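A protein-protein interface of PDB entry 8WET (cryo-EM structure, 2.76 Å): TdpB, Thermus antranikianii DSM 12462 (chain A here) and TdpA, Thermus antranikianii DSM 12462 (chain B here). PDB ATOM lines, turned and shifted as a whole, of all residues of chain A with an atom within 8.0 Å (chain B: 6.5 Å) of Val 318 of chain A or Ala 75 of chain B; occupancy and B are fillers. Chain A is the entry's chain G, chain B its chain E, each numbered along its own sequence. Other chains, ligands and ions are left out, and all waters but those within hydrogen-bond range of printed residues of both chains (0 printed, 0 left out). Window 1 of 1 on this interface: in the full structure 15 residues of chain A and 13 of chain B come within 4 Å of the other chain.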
ATOM      1  N   LEU A 280      16.663  11.561  26.282  1.00  0.00           N
ATOM      2  CA  LEU A 280      15.569  10.630  26.038  1.00  0.00           C
ATOM      3  C   LEU A 280      14.807  10.909  24.749  1.00  0.00           C
ATOM      4  O   LEU A 280      14.107  10.016  24.261  1.00  0.00           O
ATOM      5  CB  LEU A 280      14.586  10.651  27.214  1.00  0.00           C
ATOM      6  CG  LEU A 280      15.205  10.653  28.614  1.00  0.00           C
ATOM      7  CD1 LEU A 280      14.122  10.696  29.681  1.00  0.00           C
ATOM      8  CD2 LEU A 280      16.102   9.441  28.808  1.00  0.00           C
ATOM      9  N   LEU A 281      14.924  12.110  24.189  1.00  0.00           N
ATOM     10  CA  LEU A 281      14.225  12.483  22.968  1.00  0.00           C
ATOM     11  C   LEU A 281      15.226  12.944  21.918  1.00  0.00           C
ATOM     12  O   LEU A 281      16.159  13.693  22.224  1.00  0.00           O
ATOM     13  CB  LEU A 281      13.202  13.589  23.235  1.00  0.00           C
ATOM     14  CG  LEU A 281      12.186  13.325  24.347  1.00  0.00           C
ATOM     15  CD1 LEU A 281      11.423  14.593  24.686  1.00  0.00           C
ATOM     16  CD2 LEU A 281      11.230  12.215  23.950  1.00  0.00           C
ATOM     17  N   ASP A 283      14.362  14.710  19.062  1.00  0.00           N
ATOM     18  CA  ASP A 283      13.955  16.062  18.708  1.00  0.00           C
ATOM     19  C   ASP A 283      13.265  16.706  19.902  1.00  0.00           C
ATOM     20  O   ASP A 283      12.429  16.077  20.558  1.00  0.00           O
ATOM     21  CB  ASP A 283      13.023  16.055  17.496  1.00  0.00           C
ATOM     22  CG  ASP A 283      13.719  15.598  16.232  1.00  0.00           C
ATOM     23  OD1 ASP A 283      14.945  15.803  16.119  1.00  0.00           O
ATOM     24  OD2 ASP A 283      13.039  15.031  15.351  1.00  0.00           O
ATOM     25  N   PHE A 285      12.738  20.654  20.175  1.00  0.00           N
ATOM     26  CA  PHE A 285      12.257  22.022  19.976  1.00  0.00           C
ATOM     27  C   PHE A 285      13.044  23.037  20.799  1.00  0.00           C
ATOM     28  O   PHE A 285      12.843  24.246  20.646  1.00  0.00           O
ATOM     29  CB  PHE A 285      10.768  22.162  20.321  1.00  0.00           C
ATOM     30  CG  PHE A 285       9.837  21.615  19.282  1.00  0.00           C
ATOM     31  CD1 PHE A 285      10.147  21.693  17.937  1.00  0.00           C
ATOM     32  CD2 PHE A 285       8.636  21.039  19.654  1.00  0.00           C
ATOM     33  CE1 PHE A 285       9.280  21.195  16.986  1.00  0.00           C
ATOM     34  CE2 PHE A 285       7.768  20.540  18.709  1.00  0.00           C
ATOM     35  CZ  PHE A 285       8.091  20.618  17.374  1.00  0.00           C
ATOM     36  N   GLU A 289      15.879  20.370  26.361  1.00  0.00           N
ATOM     37  CA  GLU A 289      14.796  19.438  26.625  1.00  0.00           C
ATOM     38  C   GLU A 289      15.257  17.997  26.423  1.00  0.00           C
ATOM     39  O   GLU A 289      16.192  17.713  25.671  1.00  0.00           O
ATOM     40  CB  GLU A 289      13.596  19.726  25.723  1.00  0.00           C
ATOM     41  CG  GLU A 289      12.811  20.966  26.102  1.00  0.00           C
ATOM     42  CD  GLU A 289      11.446  21.002  25.448  1.00  0.00           C
ATOM     43  OE1 GLU A 289      11.041  19.975  24.866  1.00  0.00           O
ATOM     44  OE2 GLU A 289      10.779  22.054  25.516  1.00  0.00           O
ATOM     45  N   GLY A 290      14.585  17.081  27.120  1.00  0.00           N
ATOM     46  CA  GLY A 290      14.815  15.663  26.947  1.00  0.00           C
ATOM     47  C   GLY A 290      16.001  15.093  27.690  1.00  0.00           C
ATOM     48  O   GLY A 290      16.308  13.908  27.508  1.00  0.00           O
ATOM     49  N   HIS A 315      10.423   4.170  30.141  1.00  0.00           N
ATOM     50  CA  HIS A 315       9.357   4.854  30.858  1.00  0.00           C
ATOM     51  C   HIS A 315       9.276   6.333  30.509  1.00  0.00           C
ATOM     52  O   HIS A 315       8.552   7.077  31.177  1.00  0.00           O
ATOM     53  CB  HIS A 315       9.543   4.683  32.367  1.00  0.00           C
ATOM     54  CG  HIS A 315       9.190   3.318  32.867  1.00  0.00           C
ATOM     55  ND1 HIS A 315      10.082   2.267  32.855  1.00  0.00           N
ATOM     56  CD2 HIS A 315       8.043   2.831  33.395  1.00  0.00           C
ATOM     57  CE1 HIS A 315       9.500   1.192  33.353  1.00  0.00           C
ATOM     58  NE2 HIS A 315       8.262   1.507  33.689  1.00  0.00           N
ATOM     59  N   ARG A 316       9.984   6.774  29.473  1.00  0.00           N
ATOM     60  CA  ARG A 316      10.049   8.193  29.158  1.00  0.00           C
ATOM     61  C   ARG A 316       8.685   8.722  28.731  1.00  0.00           C
ATOM     62  O   ARG A 316       7.831   7.985  28.232  1.00  0.00           O
ATOM     63  CB  ARG A 316      11.076   8.451  28.055  1.00  0.00           C
ATOM     64  CG  ARG A 316      10.529   8.301  26.647  1.00  0.00           C
ATOM     65  CD  ARG A 316      11.642   8.260  25.618  1.00  0.00           C
ATOM     66  NE  ARG A 316      11.199   8.759  24.321  1.00  0.00           N
ATOM     67  CZ  ARG A 316      10.850   7.988  23.300  1.00  0.00           C
ATOM     68  NH1 ARG A 316      10.871   6.669  23.393  1.00  0.00           N
ATOM     69  NH2 ARG A 316      10.469   8.555  22.160  1.00  0.00           N
ATOM     70  N   SER A 317       8.483  10.017  28.953  1.00  0.00           N
ATOM     71  CA  SER A 317       7.245  10.689  28.595  1.00  0.00           C
ATOM     72  C   SER A 317       7.573  12.068  28.045  1.00  0.00           C
ATOM     73  O   SER A 317       8.677  12.583  28.227  1.00  0.00           O
ATOM     74  CB  SER A 317       6.298  10.809  29.797  1.00  0.00           C
ATOM     75  OG  SER A 317       5.089  11.449  29.432  1.00  0.00           O
ATOM     76  N   VAL A 318       6.600  12.660  27.366  1.00  0.00           N
ATOM     77  CA  VAL A 318       6.712  14.022  26.848  1.00  0.00           C
ATOM     78  C   VAL A 318       5.619  14.837  27.532  1.00  0.00           C
ATOM     79  O   VAL A 318       4.472  14.904  27.080  1.00  0.00           O
ATOM     80  CB  VAL A 318       6.609  14.081  25.320  1.00  0.00           C
ATOM     81  CG1 VAL A 318       7.876  13.537  24.696  1.00  0.00           C
ATOM     82  CG2 VAL A 318       5.430  13.258  24.821  1.00  0.00           C
ATOM     83  N   LEU A 319       5.968  15.470  28.650  1.00  0.00           N
ATOM     84  CA  LEU A 319       4.999  16.235  29.422  1.00  0.00           C
ATOM     85  C   LEU A 319       5.450  17.662  29.681  1.00  0.00           C
ATOM     86  O   LEU A 319       4.716  18.606  29.363  1.00  0.00           O
ATOM     87  CB  LEU A 319       4.713  15.519  30.749  1.00  0.00           C
ATOM     88  CG  LEU A 319       3.658  14.416  30.636  1.00  0.00           C
ATOM     89  CD1 LEU A 319       3.332  13.824  31.994  1.00  0.00           C
ATOM     90  CD2 LEU A 319       2.409  14.941  29.961  1.00  0.00           C
ATOM     91  N   TYR A 320       6.639  17.852  30.252  1.00  0.00           N
ATOM     92  CA  TYR A 320       7.194  19.185  30.451  1.00  0.00           C
ATOM     93  C   TYR A 320       8.448  19.398  29.616  1.00  0.00           C
ATOM     94  O   TYR A 320       8.501  20.337  28.816  1.00  0.00           O
ATOM     95  CB  TYR A 320       7.495  19.411  31.938  1.00  0.00           C
ATOM     96  CG  TYR A 320       6.380  18.985  32.865  1.00  0.00           C
ATOM     97  CD1 TYR A 320       5.189  19.695  32.923  1.00  0.00           C
ATOM     98  CD2 TYR A 320       6.517  17.869  33.677  1.00  0.00           C
ATOM     99  CE1 TYR A 320       4.168  19.306  33.769  1.00  0.00           C
ATOM    100  CE2 TYR A 320       5.502  17.474  34.523  1.00  0.00           C
ATOM    101  CZ  TYR A 320       4.330  18.195  34.566  1.00  0.00           C
ATOM    102  OH  TYR A 320       3.318  17.801  35.409  1.00  0.00           O
ATOM    103  N   GLY A 321       9.459  18.551  29.778  1.00  0.00           N
ATOM    104  CA  GLY A 321      10.663  18.621  28.978  1.00  0.00           C
ATOM    105  C   GLY A 321      11.228  17.245  28.695  1.00  0.00           C
ATOM    106  O   GLY A 321      12.445  17.082  28.571  1.00  0.00           O
ATOM    107  N   GLY A 322      10.355  16.247  28.597  1.00  0.00           N
ATOM    108  CA  GLY A 322      10.801  14.873  28.486  1.00  0.00           C
ATOM    109  C   GLY A 322      11.196  14.288  29.826  1.00  0.00           C
ATOM    110  O   GLY A 322      12.355  13.917  30.034  1.00  0.00           O
ATOM    111  N   SER A 323      10.237  14.199  30.744  1.00  0.00           N
ATOM    112  CA  SER A 323      10.500  13.722  32.095  1.00  0.00           C
ATOM    113  C   SER A 323      10.545  12.194  32.113  1.00  0.00           C
ATOM    114  O   SER A 323      10.551  11.532  31.071  1.00  0.00           O
ATOM    115  CB  SER A 323       9.453  14.272  33.060  1.00  0.00           C
ATOM    116  OG  SER A 323       9.597  15.672  33.227  1.00  0.00           O
ATOM    117  N   VAL A 324      10.574  11.614  33.317  1.00  0.00           N
ATOM    118  CA  VAL A 324      10.692  10.167  33.470  1.00  0.00           C
ATOM    119  C   VAL A 324       9.327   9.488  33.531  1.00  0.00           C
ATOM    120  O   VAL A 324       9.249   8.252  33.460  1.00  0.00           O
ATOM    121  CB  VAL A 324      11.561   9.874  34.714  1.00  0.00           C
ATOM    122  CG1 VAL A 324      11.688   8.380  35.003  1.00  0.00           C
ATOM    123  CG2 VAL A 324      12.938  10.501  34.552  1.00  0.00           C
ATOM    124  N   GLY A 325       8.242  10.252  33.613  1.00  0.00           N
ATOM    125  CA  GLY A 325       6.918   9.668  33.560  1.00  0.00           C
ATOM    126  C   GLY A 325       6.418   9.161  34.897  1.00  0.00           C
ATOM    127  O   GLY A 325       5.432   9.677  35.430  1.00  0.00           O
ATOM    128  N   TYR B  70       1.543  21.856  22.338  1.00  0.00           N
ATOM    129  CA  TYR B  70       2.974  21.608  22.480  1.00  0.00           C
ATOM    130  C   TYR B  70       3.256  20.141  22.775  1.00  0.00           C
ATOM    131  O   TYR B  70       4.187  19.554  22.210  1.00  0.00           O
ATOM    132  CB  TYR B  70       3.557  22.497  23.577  1.00  0.00           C
ATOM    133  CG  TYR B  70       5.068  22.517  23.601  1.00  0.00           C
ATOM    134  CD1 TYR B  70       5.784  23.347  22.752  1.00  0.00           C
ATOM    135  CD2 TYR B  70       5.777  21.703  24.472  1.00  0.00           C
ATOM    136  CE1 TYR B  70       7.164  23.365  22.770  1.00  0.00           C
ATOM    137  CE2 TYR B  70       7.156  21.714  24.498  1.00  0.00           C
ATOM    138  CZ  TYR B  70       7.844  22.546  23.646  1.00  0.00           C
ATOM    139  OH  TYR B  70       9.219  22.560  23.669  1.00  0.00           O
ATOM    140  N   THR B  71       2.465  19.532  23.661  1.00  0.00           N
ATOM    141  CA  THR B  71       2.667  18.126  23.994  1.00  0.00           C
ATOM    142  C   THR B  71       2.463  17.235  22.776  1.00  0.00           C
ATOM    143  O   THR B  71       3.269  16.333  22.514  1.00  0.00           O
ATOM    144  CB  THR B  71       1.723  17.717  25.126  1.00  0.00           C
ATOM    145  OG1 THR B  71       2.176  18.290  26.357  1.00  0.00           O
ATOM    146  CG2 THR B  71       1.672  16.206  25.270  1.00  0.00           C
ATOM    147  N   LEU B  72       1.401  17.484  22.006  1.00  0.00           N
ATOM    148  CA  LEU B  72       1.139  16.672  20.823  1.00  0.00           C
ATOM    149  C   LEU B  72       2.208  16.880  19.755  1.00  0.00           C
ATOM    150  O   LEU B  72       2.631  15.920  19.105  1.00  0.00           O
ATOM    151  CB  LEU B  72      -0.253  16.982  20.272  1.00  0.00           C
ATOM    152  CG  LEU B  72      -1.417  16.368  21.055  1.00  0.00           C
ATOM    153  CD1 LEU B  72      -2.739  16.980  20.632  1.00  0.00           C
ATOM    154  CD2 LEU B  72      -1.444  14.859  20.883  1.00  0.00           C
ATOM    155  N   ALA B  73       2.668  18.119  19.567  1.00  0.00           N
ATOM    156  CA  ALA B  73       3.724  18.366  18.589  1.00  0.00           C
ATOM    157  C   ALA B  73       5.023  17.677  18.988  1.00  0.00           C
ATOM    158  O   ALA B  73       5.715  17.098  18.140  1.00  0.00           O
ATOM    159  CB  ALA B  73       3.941  19.870  18.422  1.00  0.00           C
ATOM    160  N   LEU B  74       5.376  17.734  20.276  1.00  0.00           N
ATOM    161  CA  LEU B  74       6.583  17.063  20.746  1.00  0.00           C
ATOM    162  C   LEU B  74       6.465  15.551  20.601  1.00  0.00           C
ATOM    163  O   LEU B  74       7.432  14.882  20.222  1.00  0.00           O
ATOM    164  CB  LEU B  74       6.864  17.448  22.197  1.00  0.00           C
ATOM    165  CG  LEU B  74       8.248  17.112  22.755  1.00  0.00           C
ATOM    166  CD1 LEU B  74       9.334  17.778  21.932  1.00  0.00           C
ATOM    167  CD2 LEU B  74       8.349  17.532  24.210  1.00  0.00           C
ATOM    168  N   ALA B  75       5.290  14.994  20.900  1.00  0.00           N
ATOM    169  CA  ALA B  75       5.082  13.563  20.722  1.00  0.00           C
ATOM    170  C   ALA B  75       4.983  13.170  19.255  1.00  0.00           C
ATOM    171  O   ALA B  75       5.082  11.982  18.938  1.00  0.00           O
ATOM    172  CB  ALA B  75       3.822  13.118  21.465  1.00  0.00           C
ATOM    173  N   HIS B  76       4.762  14.133  18.360  1.00  0.00           N
ATOM    174  CA  HIS B  76       4.702  13.854  16.931  1.00  0.00           C
ATOM    175  C   HIS B  76       6.071  13.902  16.263  1.00  0.00           C
ATOM    176  O   HIS B  76       6.378  13.041  15.432  1.00  0.00           O
ATOM    177  CB  HIS B  76       3.758  14.842  16.240  1.00  0.00           C
ATOM    178  CG  HIS B  76       3.884  14.855  14.749  1.00  0.00           C
ATOM    179  ND1 HIS B  76       3.273  13.921  13.941  1.00  0.00           N
ATOM    180  CD2 HIS B  76       4.550  15.693  13.919  1.00  0.00           C
ATOM    181  CE1 HIS B  76       3.559  14.181  12.678  1.00  0.00           C
ATOM    182  NE2 HIS B  76       4.331  15.250  12.637  1.00  0.00           N
ATOM    183  N   ILE B  77       6.903  14.893  16.600  1.00  0.00           N
ATOM    184  CA  ILE B  77       8.214  14.993  15.961  1.00  0.00           C
ATOM    185  C   ILE B  77       9.057  13.766  16.285  1.00  0.00           C
ATOM    186  O   ILE B  77       9.828  13.285  15.445  1.00  0.00           O
ATOM    187  CB  ILE B  77       8.923  16.302  16.360  1.00  0.00           C
ATOM    188  CG1 ILE B  77       9.076  16.409  17.876  1.00  0.00           C
ATOM    189  CG2 ILE B  77       8.161  17.494  15.816  1.00  0.00           C
ATOM    190  CD1 ILE B  77       9.885  17.606  18.317  1.00  0.00           C
ATOM    191  N   ASN B  78       8.931  13.246  17.500  1.00  0.00           N
ATOM    192  CA  ASN B  78       9.419  11.910  17.800  1.00  0.00           C
ATOM    193  C   ASN B  78       8.367  10.886  17.397  1.00  0.00           C
ATOM    194  O   ASN B  78       7.163  11.135  17.489  1.00  0.00           O
ATOM    195  CB  ASN B  78       9.744  11.770  19.287  1.00  0.00           C
ATOM    196  CG  ASN B  78      10.470  12.976  19.841  1.00  0.00           C
ATOM    197  OD1 ASN B  78      11.682  13.109  19.684  1.00  0.00           O
ATOM    198  ND2 ASN B  78       9.732  13.864  20.492  1.00  0.00           N
ATOM    199  N   GLN B  79       8.826   9.725  16.936  1.00  0.00           N
ATOM    200  CA  GLN B  79       7.912   8.663  16.516  1.00  0.00           C
ATOM    201  C   GLN B  79       7.328   7.988  17.758  1.00  0.00           C
ATOM    202  O   GLN B  79       7.607   6.831  18.081  1.00  0.00           O
ATOM    203  CB  GLN B  79       8.620   7.671  15.606  1.00  0.00           C
ATOM    204  CG  GLN B  79       8.828   8.171  14.181  1.00  0.00           C
ATOM    205  CD  GLN B  79       9.867   9.270  14.087  1.00  0.00           C
ATOM    206  OE1 GLN B  79       9.566  10.390  13.675  1.00  0.00           O
ATOM    207  NE2 GLN B  79      11.098   8.955  14.470  1.00  0.00           N
ATOM    208  N   VAL B  80       6.498   8.748  18.465  1.00  0.00           N
ATOM    209  CA  VAL B  80       5.846   8.290  19.686  1.00  0.00           C
ATOM    210  C   VAL B  80       4.417   7.907  19.329  1.00  0.00           C
ATOM    211  O   VAL B  80       3.607   8.762  18.959  1.00  0.00           O
ATOM    212  CB  VAL B  80       5.880   9.360  20.785  1.00  0.00           C
ATOM    213  CG1 VAL B  80       4.934   8.990  21.916  1.00  0.00           C
ATOM    214  CG2 VAL B  80       7.295   9.539  21.308  1.00  0.00           C
ATOM    215  N   ASP B  81       4.106   6.619  19.441  1.00  0.00           N
ATOM    216  CA  ASP B  81       2.755   6.119  19.200  1.00  0.00           C
ATOM    217  C   ASP B  81       1.988   6.226  20.509  1.00  0.00           C
ATOM    218  O   ASP B  81       2.209   5.445  21.437  1.00  0.00           O
ATOM    219  CB  ASP B  81       2.790   4.687  18.680  1.00  0.00           C
ATOM    220  CG  ASP B  81       1.416   4.169  18.304  1.00  0.00           C
ATOM    221  OD1 ASP B  81       0.498   4.994  18.116  1.00  0.00           O
ATOM    222  OD2 ASP B  81       1.256   2.935  18.193  1.00  0.00           O
ATOM    223  N   LEU B  82       1.075   7.195  20.585  1.00  0.00           N
ATOM    224  CA  LEU B  82       0.336   7.433  21.817  1.00  0.00           C
ATOM    225  C   LEU B  82      -0.641   6.314  22.145  1.00  0.00           C
ATOM    226  O   LEU B  82      -1.216   6.324  23.239  1.00  0.00           O
ATOM    227  CB  LEU B  82      -0.410   8.765  21.740  1.00  0.00           C
ATOM    228  CG  LEU B  82       0.422   9.998  22.101  1.00  0.00           C
ATOM    229  CD1 LEU B  82      -0.449  11.240  22.163  1.00  0.00           C
ATOM    230  CD2 LEU B  82       1.151   9.783  23.416  1.00  0.00           C
ATOM    231  N   ASP B  86       3.129   6.113  25.801  1.00  0.00           N
ATOM    232  CA  ASP B  86       3.159   7.184  26.798  1.00  0.00           C
ATOM    233  C   ASP B  86       1.788   7.318  27.440  1.00  0.00           C
ATOM    234  O   ASP B  86       0.998   8.200  27.082  1.00  0.00           O
ATOM    235  CB  ASP B  86       3.599   8.505  26.162  1.00  0.00           C
ATOM    236  CG  ASP B  86       3.985   9.548  27.186  1.00  0.00           C
ATOM    237  OD1 ASP B  86       3.802   9.298  28.395  1.00  0.00           O
ATOM    238  OD2 ASP B  86       4.475  10.622  26.780  1.00  0.00           O
ATOM    239  N   ALA B  89       0.991  10.982  29.099  1.00  0.00           N
ATOM    240  CA  ALA B  89       0.642  12.104  28.233  1.00  0.00           C
ATOM    241  C   ALA B  89      -0.749  11.930  27.639  1.00  0.00           C
ATOM    242  O   ALA B  89      -1.464  12.914  27.421  1.00  0.00           O
ATOM    243  CB  ALA B  89       1.682  12.260  27.126  1.00  0.00           C
ATOM    244  N   GLU B  92      -3.972  13.126  30.008  1.00  0.00           N
ATOM    245  CA  GLU B  92      -4.342  14.501  30.306  1.00  0.00           C
ATOM    246  C   GLU B  92      -4.873  15.266  29.104  1.00  0.00           C
ATOM    247  O   GLU B  92      -5.376  16.381  29.281  1.00  0.00           O
ATOM    248  CB  GLU B  92      -3.153  15.280  30.883  1.00  0.00           C
ATOM    249  CG  GLU B  92      -2.073  15.596  29.873  1.00  0.00           C
ATOM    250  CD  GLU B  92      -0.955  16.421  30.469  1.00  0.00           C
ATOM    251  OE1 GLU B  92      -0.992  16.682  31.690  1.00  0.00           O
ATOM    252  OE2 GLU B  92      -0.058  16.843  29.710  1.00  0.00           O
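The backbone NH (N) of Asp 283 of chain A is in hydrogen-bond range of the side-chain amide oxygen (OD1) of Asn 78 of chain B. The side-chain carboxylate (OE2) of Glu 289 of chain A lies within hydrogen-bond range of the side-chain hydroxyl (OH) of Tyr 70 of chain B, at 2.5 Å. The side-chain hydroxyl (OG) of Ser 317 of chain A lies within hydrogen-bond range of the side-chain carboxylate (OD1) of Asp 86 of chain B, 2.7 Å away. OD2 of Asp 86 of chain B is in hydrogen-bond range of N of Val 318 of chain A (3.0 Å).
The backbone carbonyl oxygen (O) of Leu 280 of chain A is in hydrogen-bond range of the guanidinium group (NE) of Arg 316 of chain A (3.2 Å). N of Ser 317 of chain A is in hydrogen-bond range of O of Ser 323 of chain A. The backbone carbonyl oxygen (O) of Leu 74 of chain B sits at hydrogen-bond distance from the side-chain amide nitrogen (ND2) of Asn 78 of chain B (2.5 Å). The backbone carbonyl oxygen (O) of Ile 77 of chain B lies close to the side-chain amide oxygen (OE1) of Gln 79 of chain B (3.4 Å). The backbone NH (N) of Ala 89 of chain B sits at hydrogen-bond distance from the side-chain carboxylate (OD1) of Asp 86 of chain B (3.4 Å).
Leu 281 of chain A touches Asn 78 of chain B. Leu 74 of chain B touches Asp 283 of chain A. Asp 283 of chain A touches Ile 77 of chain B (CB to CD1, 3.6 Å). CB of Phe 285 of chain A touches OH of Tyr 70 of chain B (3.7 Å). CZ of Phe 285 of chain A touches CG2 of Ile 77 of chain B (3.5 Å). Glu 289 of chain A touches Leu 74 of chain B. Arg 316 of chain A touches Val 80 of chain B. Val 318 of chain A touches Thr 71 of chain B (O to CG2, 3.6 Å). CD2 of Leu 319 of chain A touches CA of Ala 89 of chain B (3.8 Å). Leu 319 of chain A touches Glu 92 of chain B (CD2 to OE2, 3.1 Å).
His 315 of chain A touches none of the printed residues of chain B. Of the printed residues of chain B, Ser 317 of chain A touches Asp 86 (2.7 Å). Of chain B, only Thr 71 (3.6 Å), Ala 75 (3.7 Å), Asp 86 (3.0 Å) and Ala 89 (3.8 Å) come within 4 Å of Val 318 of chain A. Of the printed residues of chain A, Thr 71 of chain B touches Val 318 and Leu 319. Of chain A, only Val 318 (3.7 Å) comes within 4 Å of Ala 75 of chain B. Printed residues of chain A within 4 Å of Ala 89 of chain B: Val 318 (3.8 Å) and Leu 319 (3.8 Å).
Printed residues of chain B that touch a printed residue of chain A: Tyr 70, Thr 71, Ala 73, Leu 74, Ala 75, Ile 77, Asn 78, Val 80, Asp 86, Ala 89 and Glu 92. Hydrophobic or aromatic side chains of chain B that line the printed part of chain A: Tyr 70, Ala 73, Leu 74, Ala 75, Ile 77, Val 80 and Ala 89. Hydrophobic or aromatic side chains of chain A within 4 Å of the printed part of chain B: Leu 281, Phe 285, Val 318 and Leu 319. Along chain A the printed residues that touch a printed residue of chain B span positions 281 to 319. Among the printed residues, no Asp or Glu carboxylate lies within 4 Å of a Lys or Arg side-chain nitrogen of the other chain.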
